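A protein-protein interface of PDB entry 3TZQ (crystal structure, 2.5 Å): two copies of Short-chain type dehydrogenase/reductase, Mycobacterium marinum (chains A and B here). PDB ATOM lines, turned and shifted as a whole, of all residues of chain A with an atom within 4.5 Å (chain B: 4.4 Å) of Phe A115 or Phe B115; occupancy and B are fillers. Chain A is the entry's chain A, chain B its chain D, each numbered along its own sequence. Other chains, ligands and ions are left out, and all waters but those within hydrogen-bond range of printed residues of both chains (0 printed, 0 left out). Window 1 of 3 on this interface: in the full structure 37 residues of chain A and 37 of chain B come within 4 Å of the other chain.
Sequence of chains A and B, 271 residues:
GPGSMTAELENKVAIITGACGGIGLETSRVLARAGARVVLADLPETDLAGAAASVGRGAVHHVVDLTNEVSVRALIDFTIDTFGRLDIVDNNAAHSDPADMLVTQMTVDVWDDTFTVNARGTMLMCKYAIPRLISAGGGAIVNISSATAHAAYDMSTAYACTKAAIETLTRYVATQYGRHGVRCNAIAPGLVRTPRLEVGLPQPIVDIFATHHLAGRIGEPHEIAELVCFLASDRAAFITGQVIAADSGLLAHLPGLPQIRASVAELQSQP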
ATOM      1  N   TRP A 111     -20.523  -1.633  20.141  1.00  0.00           N
ATOM      2  CA  TRP A 111     -19.959  -0.300  20.345  1.00  0.00           C
ATOM      3  C   TRP A 111     -18.641  -0.160  19.617  1.00  0.00           C
ATOM      4  O   TRP A 111     -18.501   0.761  18.814  1.00  0.00           O
ATOM      5  CB  TRP A 111     -19.815  -0.014  21.845  1.00  0.00           C
ATOM      6  CG  TRP A 111     -19.331   1.378  22.206  1.00  0.00           C
ATOM      7  CD1 TRP A 111     -18.010   1.796  22.376  1.00  0.00           C
ATOM      8  CD2 TRP A 111     -20.144   2.581  22.480  1.00  0.00           C
ATOM      9  NE1 TRP A 111     -17.954   3.116  22.717  1.00  0.00           N
ATOM     10  CE2 TRP A 111     -19.195   3.647  22.806  1.00  0.00           C
ATOM     11  CE3 TRP A 111     -21.500   2.863  22.493  1.00  0.00           C
ATOM     12  CZ2 TRP A 111     -19.610   4.939  23.102  1.00  0.00           C
ATOM     13  CZ3 TRP A 111     -21.913   4.170  22.805  1.00  0.00           C
ATOM     14  CH2 TRP A 111     -20.987   5.184  23.098  1.00  0.00           C
ATOM     15  N   ASP A 112     -17.685  -1.069  19.853  1.00  0.00           N
ATOM     16  CA  ASP A 112     -16.327  -0.935  19.267  1.00  0.00           C
ATOM     17  C   ASP A 112     -16.310  -1.112  17.740  1.00  0.00           C
ATOM     18  O   ASP A 112     -15.572  -0.401  17.027  1.00  0.00           O
ATOM     19  CB  ASP A 112     -15.306  -1.904  19.909  1.00  0.00           C
ATOM     20  CG  ASP A 112     -14.890  -1.493  21.334  1.00  0.00           C
ATOM     21  OD1 ASP A 112     -15.235  -0.385  21.772  1.00  0.00           O
ATOM     22  OD2 ASP A 112     -14.220  -2.278  22.041  1.00  0.00           O
ATOM     23  N   ASP A 113     -17.100  -2.055  17.232  1.00  0.00           N
ATOM     24  CA  ASP A 113     -17.205  -2.229  15.795  1.00  0.00           C
ATOM     25  C   ASP A 113     -17.632  -0.926  15.146  1.00  0.00           C
ATOM     26  O   ASP A 113     -17.126  -0.577  14.076  1.00  0.00           O
ATOM     27  CB  ASP A 113     -18.232  -3.292  15.425  1.00  0.00           C
ATOM     28  CG  ASP A 113     -17.748  -4.694  15.651  1.00  0.00           C
ATOM     29  OD1 ASP A 113     -16.539  -4.879  15.882  1.00  0.00           O
ATOM     30  OD2 ASP A 113     -18.590  -5.614  15.583  1.00  0.00           O
ATOM     31  N   THR A 114     -18.563  -0.212  15.785  1.00  0.00           N
ATOM     32  CA  THR A 114     -19.152   0.985  15.191  1.00  0.00           C
ATOM     33  C   THR A 114     -18.181   2.173  15.240  1.00  0.00           C
ATOM     34  O   THR A 114     -18.074   2.929  14.280  1.00  0.00           O
ATOM     35  CB  THR A 114     -20.517   1.319  15.829  1.00  0.00           C
ATOM     36  OG1 THR A 114     -21.368   0.173  15.756  1.00  0.00           O
ATOM     37  CG2 THR A 114     -21.202   2.467  15.120  1.00  0.00           C
ATOM     38  N   PHE A 115     -17.451   2.324  16.336  1.00  0.00           N
ATOM     39  CA  PHE A 115     -16.454   3.408  16.447  1.00  0.00           C
ATOM     40  C   PHE A 115     -15.234   3.188  15.558  1.00  0.00           C
ATOM     41  O   PHE A 115     -14.744   4.127  14.924  1.00  0.00           O
ATOM     42  CB  PHE A 115     -16.024   3.615  17.903  1.00  0.00           C
ATOM     43  CG  PHE A 115     -16.917   4.568  18.663  1.00  0.00           C
ATOM     44  CD1 PHE A 115     -18.100   4.120  19.241  1.00  0.00           C
ATOM     45  CD2 PHE A 115     -16.590   5.899  18.778  1.00  0.00           C
ATOM     46  CE1 PHE A 115     -18.931   4.982  19.919  1.00  0.00           C
ATOM     47  CE2 PHE A 115     -17.413   6.766  19.459  1.00  0.00           C
ATOM     48  CZ  PHE A 115     -18.588   6.311  20.031  1.00  0.00           C
ATOM     49  N   THR A 116     -14.778   1.943  15.491  1.00  0.00           N
ATOM     50  CA  THR A 116     -13.669   1.538  14.610  1.00  0.00           C
ATOM     51  C   THR A 116     -13.904   1.900  13.147  1.00  0.00           C
ATOM     52  O   THR A 116     -13.054   2.497  12.514  1.00  0.00           O
ATOM     53  CB  THR A 116     -13.418   0.030  14.722  1.00  0.00           C
ATOM     54  OG1 THR A 116     -13.132  -0.263  16.086  1.00  0.00           O
ATOM     55  CG2 THR A 116     -12.249  -0.404  13.877  1.00  0.00           C
ATOM     56  N   VAL A 117     -15.056   1.553  12.610  1.00  0.00           N
ATOM     57  CA  VAL A 117     -15.361   1.939  11.247  1.00  0.00           C
ATOM     58  C   VAL A 117     -15.583   3.454  11.178  1.00  0.00           C
ATOM     59  O   VAL A 117     -14.829   4.152  10.513  1.00  0.00           O
ATOM     60  CB  VAL A 117     -16.567   1.168  10.660  1.00  0.00           C
ATOM     61  CG1 VAL A 117     -16.956   1.764   9.314  1.00  0.00           C
ATOM     62  CG2 VAL A 117     -16.266  -0.315  10.503  1.00  0.00           C
ATOM     63  N   ASN A 118     -16.574   3.954  11.902  1.00  0.00           N
ATOM     64  CA  ASN A 118     -17.051   5.336  11.704  1.00  0.00           C
ATOM     65  C   ASN A 118     -16.135   6.461  12.199  1.00  0.00           C
ATOM     66  O   ASN A 118     -15.860   7.400  11.467  1.00  0.00           O
ATOM     67  CB  ASN A 118     -18.414   5.550  12.368  1.00  0.00           C
ATOM     68  CG  ASN A 118     -19.479   4.626  11.843  1.00  0.00           C
ATOM     69  OD1 ASN A 118     -19.313   4.008  10.799  1.00  0.00           O
ATOM     70  ND2 ASN A 118     -20.598   4.540  12.556  1.00  0.00           N
ATOM     71  N   ALA A 119     -15.726   6.409  13.459  1.00  0.00           N
ATOM     72  CA  ALA A 119     -14.915   7.483  14.014  1.00  0.00           C
ATOM     73  C   ALA A 119     -13.463   7.252  13.621  1.00  0.00           C
ATOM     74  O   ALA A 119     -12.864   8.077  12.931  1.00  0.00           O
ATOM     75  CB  ALA A 119     -15.080   7.567  15.531  1.00  0.00           C
ATOM     76  N   ARG A 120     -12.898   6.116  14.012  1.00  0.00           N
ATOM     77  CA  ARG A 120     -11.513   5.890  13.687  1.00  0.00           C
ATOM     78  C   ARG A 120     -11.215   5.901  12.186  1.00  0.00           C
ATOM     79  O   ARG A 120     -10.252   6.528  11.722  1.00  0.00           O
ATOM     80  CB  ARG A 120     -10.994   4.596  14.297  1.00  0.00           C
ATOM     81  CG  ARG A 120      -9.505   4.685  14.575  1.00  0.00           C
ATOM     82  CD  ARG A 120      -9.017   3.434  15.254  1.00  0.00           C
ATOM     83  NE  ARG A 120      -8.833   2.397  14.266  1.00  0.00           N
ATOM     84  CZ  ARG A 120      -8.357   1.195  14.509  1.00  0.00           C
ATOM     85  NH1 ARG A 120      -8.024   0.824  15.713  1.00  0.00           N
ATOM     86  NH2 ARG A 120      -8.270   0.354  13.521  1.00  0.00           N
ATOM     87  N   ALA A 158     -24.687   3.973  19.522  1.00  0.00           N
ATOM     88  CA  ALA A 158     -23.290   3.927  19.092  1.00  0.00           C
ATOM     89  C   ALA A 158     -23.110   4.733  17.833  1.00  0.00           C
ATOM     90  O   ALA A 158     -22.303   5.655  17.778  1.00  0.00           O
ATOM     91  CB  ALA A 158     -22.864   2.495  18.839  1.00  0.00           C
ATOM     92  N   CYS A 161     -23.355   8.439  18.325  1.00  0.00           N
ATOM     93  CA  CYS A 161     -22.227   9.013  19.062  1.00  0.00           C
ATOM     94  C   CYS A 161     -20.978   9.122  18.157  1.00  0.00           C
ATOM     95  O   CYS A 161     -20.203  10.072  18.274  1.00  0.00           O
ATOM     96  CB  CYS A 161     -21.935   8.189  20.317  1.00  0.00           C
ATOM     97  SG  CYS A 161     -23.249   8.204  21.577  1.00  0.00           S
ATOM     98  N   THR A 162     -20.821   8.163  17.232  1.00  0.00           N
ATOM     99  CA  THR A 162     -19.720   8.220  16.270  1.00  0.00           C
ATOM    100  C   THR A 162     -19.915   9.402  15.317  1.00  0.00           C
ATOM    101  O   THR A 162     -18.956  10.095  14.968  1.00  0.00           O
ATOM    102  CB  THR A 162     -19.531   6.906  15.484  1.00  0.00           C
ATOM    103  OG1 THR A 162     -20.634   6.669  14.584  1.00  0.00           O
ATOM    104  CG2 THR A 162     -19.352   5.708  16.461  1.00  0.00           C
ATOM    105  N   ALA A 165     -18.626  12.405  17.065  1.00  0.00           N
ATOM    106  CA  ALA A 165     -17.143  12.394  17.002  1.00  0.00           C
ATOM    107  C   ALA A 165     -16.664  12.952  15.671  1.00  0.00           C
ATOM    108  O   ALA A 165     -15.673  13.702  15.616  1.00  0.00           O
ATOM    109  CB  ALA A 165     -16.580  10.987  17.223  1.00  0.00           C
ATOM    110  N   TRP B 111      -5.542   7.231  19.646  1.00  0.00           N
ATOM    111  CA  TRP B 111      -6.969   7.373  19.395  1.00  0.00           C
ATOM    112  C   TRP B 111      -7.770   6.391  20.223  1.00  0.00           C
ATOM    113  O   TRP B 111      -8.650   6.792  20.957  1.00  0.00           O
ATOM    114  CB  TRP B 111      -7.238   7.211  17.892  1.00  0.00           C
ATOM    115  CG  TRP B 111      -8.638   7.503  17.451  1.00  0.00           C
ATOM    116  CD1 TRP B 111      -9.669   6.590  17.274  1.00  0.00           C
ATOM    117  CD2 TRP B 111      -9.210   8.797  17.082  1.00  0.00           C
ATOM    118  NE1 TRP B 111     -10.811   7.213  16.841  1.00  0.00           N
ATOM    119  CE2 TRP B 111     -10.608   8.537  16.714  1.00  0.00           C
ATOM    120  CE3 TRP B 111      -8.729  10.106  17.026  1.00  0.00           C
ATOM    121  CZ2 TRP B 111     -11.465   9.557  16.304  1.00  0.00           C
ATOM    122  CZ3 TRP B 111      -9.599  11.120  16.630  1.00  0.00           C
ATOM    123  CH2 TRP B 111     -10.935  10.855  16.279  1.00  0.00           C
ATOM    124  N   ASP B 112      -7.437   5.106  20.166  1.00  0.00           N
ATOM    125  CA  ASP B 112      -8.197   4.078  20.870  1.00  0.00           C
ATOM    126  C   ASP B 112      -8.026   4.102  22.379  1.00  0.00           C
ATOM    127  O   ASP B 112      -9.001   3.880  23.130  1.00  0.00           O
ATOM    128  CB  ASP B 112      -7.808   2.707  20.350  1.00  0.00           C
ATOM    129  CG  ASP B 112      -8.234   2.497  18.921  1.00  0.00           C
ATOM    130  OD1 ASP B 112      -9.114   3.251  18.446  1.00  0.00           O
ATOM    131  OD2 ASP B 112      -7.704   1.576  18.271  1.00  0.00           O
ATOM    132  N   ASP B 113      -6.802   4.339  22.857  1.00  0.00           N
ATOM    133  CA  ASP B 113      -6.613   4.485  24.289  1.00  0.00           C
ATOM    134  C   ASP B 113      -7.663   5.481  24.776  1.00  0.00           C
ATOM    135  O   ASP B 113      -8.481   5.138  25.630  1.00  0.00           O
ATOM    136  CB  ASP B 113      -5.196   4.956  24.620  1.00  0.00           C
ATOM    137  CG  ASP B 113      -4.171   3.826  24.565  1.00  0.00           C
ATOM    138  OD1 ASP B 113      -4.539   2.677  24.229  1.00  0.00           O
ATOM    139  OD2 ASP B 113      -2.986   4.095  24.862  1.00  0.00           O
ATOM    140  N   THR B 114      -7.682   6.656  24.148  1.00  0.00           N
ATOM    141  CA  THR B 114      -8.551   7.790  24.517  1.00  0.00           C
ATOM    142  C   THR B 114     -10.049   7.465  24.411  1.00  0.00           C
ATOM    143  O   THR B 114     -10.830   7.867  25.270  1.00  0.00           O
ATOM    144  CB  THR B 114      -8.235   9.041  23.620  1.00  0.00           C
ATOM    145  OG1 THR B 114      -6.835   9.374  23.706  1.00  0.00           O
ATOM    146  CG2 THR B 114      -9.061  10.259  23.995  1.00  0.00           C
ATOM    147  N   PHE B 115     -10.438   6.777  23.337  1.00  0.00           N
ATOM    148  CA  PHE B 115     -11.843   6.448  23.091  1.00  0.00           C
ATOM    149  C   PHE B 115     -12.307   5.332  24.035  1.00  0.00           C
ATOM    150  O   PHE B 115     -13.418   5.368  24.523  1.00  0.00           O
ATOM    151  CB  PHE B 115     -12.098   6.073  21.607  1.00  0.00           C
ATOM    152  CG  PHE B 115     -12.581   7.233  20.758  1.00  0.00           C
ATOM    153  CD1 PHE B 115     -11.674   8.147  20.195  1.00  0.00           C
ATOM    154  CD2 PHE B 115     -13.947   7.429  20.520  1.00  0.00           C
ATOM    155  CE1 PHE B 115     -12.124   9.220  19.431  1.00  0.00           C
ATOM    156  CE2 PHE B 115     -14.383   8.506  19.748  1.00  0.00           C
ATOM    157  CZ  PHE B 115     -13.474   9.400  19.205  1.00  0.00           C
ATOM    158  N   THR B 116     -11.435   4.361  24.284  1.00  0.00           N
ATOM    159  CA  THR B 116     -11.685   3.315  25.263  1.00  0.00           C
ATOM    160  C   THR B 116     -11.955   3.885  26.673  1.00  0.00           C
ATOM    161  O   THR B 116     -12.920   3.473  27.331  1.00  0.00           O
ATOM    162  CB  THR B 116     -10.508   2.307  25.302  1.00  0.00           C
ATOM    163  OG1 THR B 116     -10.328   1.744  23.997  1.00  0.00           O
ATOM    164  CG2 THR B 116     -10.776   1.173  26.281  1.00  0.00           C
ATOM    165  N   VAL B 117     -11.140   4.838  27.137  1.00  0.00           N
ATOM    166  CA  VAL B 117     -11.385   5.422  28.459  1.00  0.00           C
ATOM    167  C   VAL B 117     -12.611   6.340  28.422  1.00  0.00           C
ATOM    168  O   VAL B 117     -13.577   6.113  29.126  1.00  0.00           O
ATOM    169  CB  VAL B 117     -10.161   6.207  28.993  1.00  0.00           C
ATOM    170  CG1 VAL B 117     -10.559   7.041  30.210  1.00  0.00           C
ATOM    171  CG2 VAL B 117      -8.993   5.259  29.303  1.00  0.00           C
ATOM    172  N   ASN B 118     -12.583   7.350  27.564  1.00  0.00           N
ATOM    173  CA  ASN B 118     -13.597   8.410  27.581  1.00  0.00           C
ATOM    174  C   ASN B 118     -14.993   8.003  27.038  1.00  0.00           C
ATOM    175  O   ASN B 118     -16.017   8.138  27.725  1.00  0.00           O
ATOM    176  CB  ASN B 118     -13.057   9.619  26.826  1.00  0.00           C
ATOM    177  CG  ASN B 118     -11.748  10.117  27.393  1.00  0.00           C
ATOM    178  OD1 ASN B 118     -11.293   9.642  28.428  1.00  0.00           O
ATOM    179  ND2 ASN B 118     -11.136  11.075  26.727  1.00  0.00           N
ATOM    180  N   ALA B 119     -15.032   7.511  25.809  1.00  0.00           N
ATOM    181  CA  ALA B 119     -16.294   7.216  25.138  1.00  0.00           C
ATOM    182  C   ALA B 119     -16.843   5.880  25.630  1.00  0.00           C
ATOM    183  O   ALA B 119     -17.914   5.809  26.222  1.00  0.00           O
ATOM    184  CB  ALA B 119     -16.088   7.178  23.626  1.00  0.00           C
ATOM    185  N   ARG B 120     -16.092   4.814  25.397  1.00  0.00           N
ATOM    186  CA  ARG B 120     -16.554   3.522  25.809  1.00  0.00           C
ATOM    187  C   ARG B 120     -16.740   3.426  27.325  1.00  0.00           C
ATOM    188  O   ARG B 120     -17.715   2.863  27.795  1.00  0.00           O
ATOM    189  CB  ARG B 120     -15.612   2.433  25.309  1.00  0.00           C
ATOM    190  CG  ARG B 120     -16.227   1.074  25.427  1.00  0.00           C
ATOM    191  CD  ARG B 120     -15.313   0.052  24.836  1.00  0.00           C
ATOM    192  NE  ARG B 120     -14.397  -0.418  25.848  1.00  0.00           N
ATOM    193  CZ  ARG B 120     -13.798  -1.595  25.824  1.00  0.00           C
ATOM    194  NH1 ARG B 120     -14.002  -2.456  24.832  1.00  0.00           N
ATOM    195  NH2 ARG B 120     -12.979  -1.904  26.818  1.00  0.00           N
ATOM    196  N   ALA B 158      -8.310  13.753  19.450  1.00  0.00           N
ATOM    197  CA  ALA B 158      -8.935  12.521  19.935  1.00  0.00           C
ATOM    198  C   ALA B 158      -9.809  12.840  21.166  1.00  0.00           C
ATOM    199  O   ALA B 158     -11.035  12.537  21.209  1.00  0.00           O
ATOM    200  CB  ALA B 158      -7.876  11.478  20.242  1.00  0.00           C
ATOM    201  N   CYS B 161     -12.832  14.699  20.137  1.00  0.00           N
ATOM    202  CA  CYS B 161     -13.839  13.855  19.491  1.00  0.00           C
ATOM    203  C   CYS B 161     -14.562  12.932  20.490  1.00  0.00           C
ATOM    204  O   CYS B 161     -15.739  12.736  20.371  1.00  0.00           O
ATOM    205  CB  CYS B 161     -13.228  13.076  18.343  1.00  0.00           C
ATOM    206  SG  CYS B 161     -12.689  14.154  16.985  1.00  0.00           S
ATOM    207  N   THR B 162     -13.872  12.422  21.504  1.00  0.00           N
ATOM    208  CA  THR B 162     -14.517  11.575  22.539  1.00  0.00           C
ATOM    209  C   THR B 162     -15.567  12.358  23.348  1.00  0.00           C
ATOM    210  O   THR B 162     -16.620  11.816  23.732  1.00  0.00           O
ATOM    211  CB  THR B 162     -13.486  10.962  23.529  1.00  0.00           C
ATOM    212  OG1 THR B 162     -12.948  11.988  24.381  1.00  0.00           O
ATOM    213  CG2 THR B 162     -12.337  10.246  22.781  1.00  0.00           C
ATOM    214  N   ALA B 165     -18.687  12.642  21.564  1.00  0.00           N
ATOM    215  CA  ALA B 165     -19.392  11.385  21.671  1.00  0.00           C
ATOM    216  C   ALA B 165     -20.214  11.309  22.975  1.00  0.00           C
ATOM    217  O   ALA B 165     -21.347  10.860  22.954  1.00  0.00           O
ATOM    218  CB  ALA B 165     -18.406  10.226  21.547  1.00  0.00           C
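Among the printed residues, merely in contact across the chains: Trp A111 with Ala B119 (3.7 Å), Trp A111 with Arg B120 (3.4 Å), Phe A115 with Phe B115 (3.5 Å), Ala A119 with Trp B111 (3.9 Å) and Arg A120 with Trp B111 (3.3 Å).
The backbone carbonyl oxygen (O) of Asp A112 sits at hydrogen-bond distance from the side-chain hydroxyl (OG1) of Thr A116, at 2.6 Å.
N of Arg A120 sits at hydrogen-bond distance from O of Phe A115 (2.9 Å).
O of Asp B112 lies within hydrogen-bond range of OG1 of Thr B116.
N of Arg B120 is in hydrogen-bond range of O of Phe B115 (2.9 Å).
Of the 14 printed residues of chain B, 7 touch a printed residue of chain A.
Hydrophobic or aromatic side chains of chain B that line the printed part of chain A: Trp B111, Phe B115 and Ala B165.
Printed residues of chain A that touch a printed residue of chain B: Trp A111, Asp A112, Phe A115, Ala A119, Arg A120, Cys A161 and Ala A165.
Among the printed residues, 9 pairs touch across the chains.
Trp A111 touches Ala B119, and with the chains exchanged Ala A119 touches Trp B111.
Asp A112 touches Arg B120, and with the chains exchanged Arg A120 touches Asp B112.
Phe A115 touches its own counterpart, Phe B115.
Cys A161 touches Ala B165, and with the chains exchanged Ala A165 touches Cys B161.
Of the 9 pairs that touch across the chains among the printed residues, 9 have their exchanged pair printed and touching as well.
The guanidinium group (NH1) of Arg B120 lies within salt-bridge range of the side-chain carboxylate (OD2) of Asp A112.
NH1 of Arg A120 is in salt-bridge range of OD2 of Asp B112 (2.7 Å).
SG of Cys A161 sits at hydrogen-bond distance from O of Ala B165.
O of Ala A165 lies within hydrogen-bond range of SG of Cys B161, at 3.3 Å.
Of chain B, only Phe B115 (3.5 Å) comes within 4 Å of Phe A115.
Of the printed residues of chain A, Phe B115 touches Phe A115 (3.5 Å).
Of the printed residues of chain A, Ala B119 touches Trp A111.
Of the printed residues of chain B, Trp A111 touches Ala B119 and Arg B120.
Printed residues of chain B within 4 Å of Asp A112: Arg B120 (2.8 Å).
The nearest residue of chain B that does not touch Phe A115 is Ala B165 (4.2 Å).
The nearest printed residue of chain B that does not touch Cys A161 is Cys B161 (5.6 Å).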
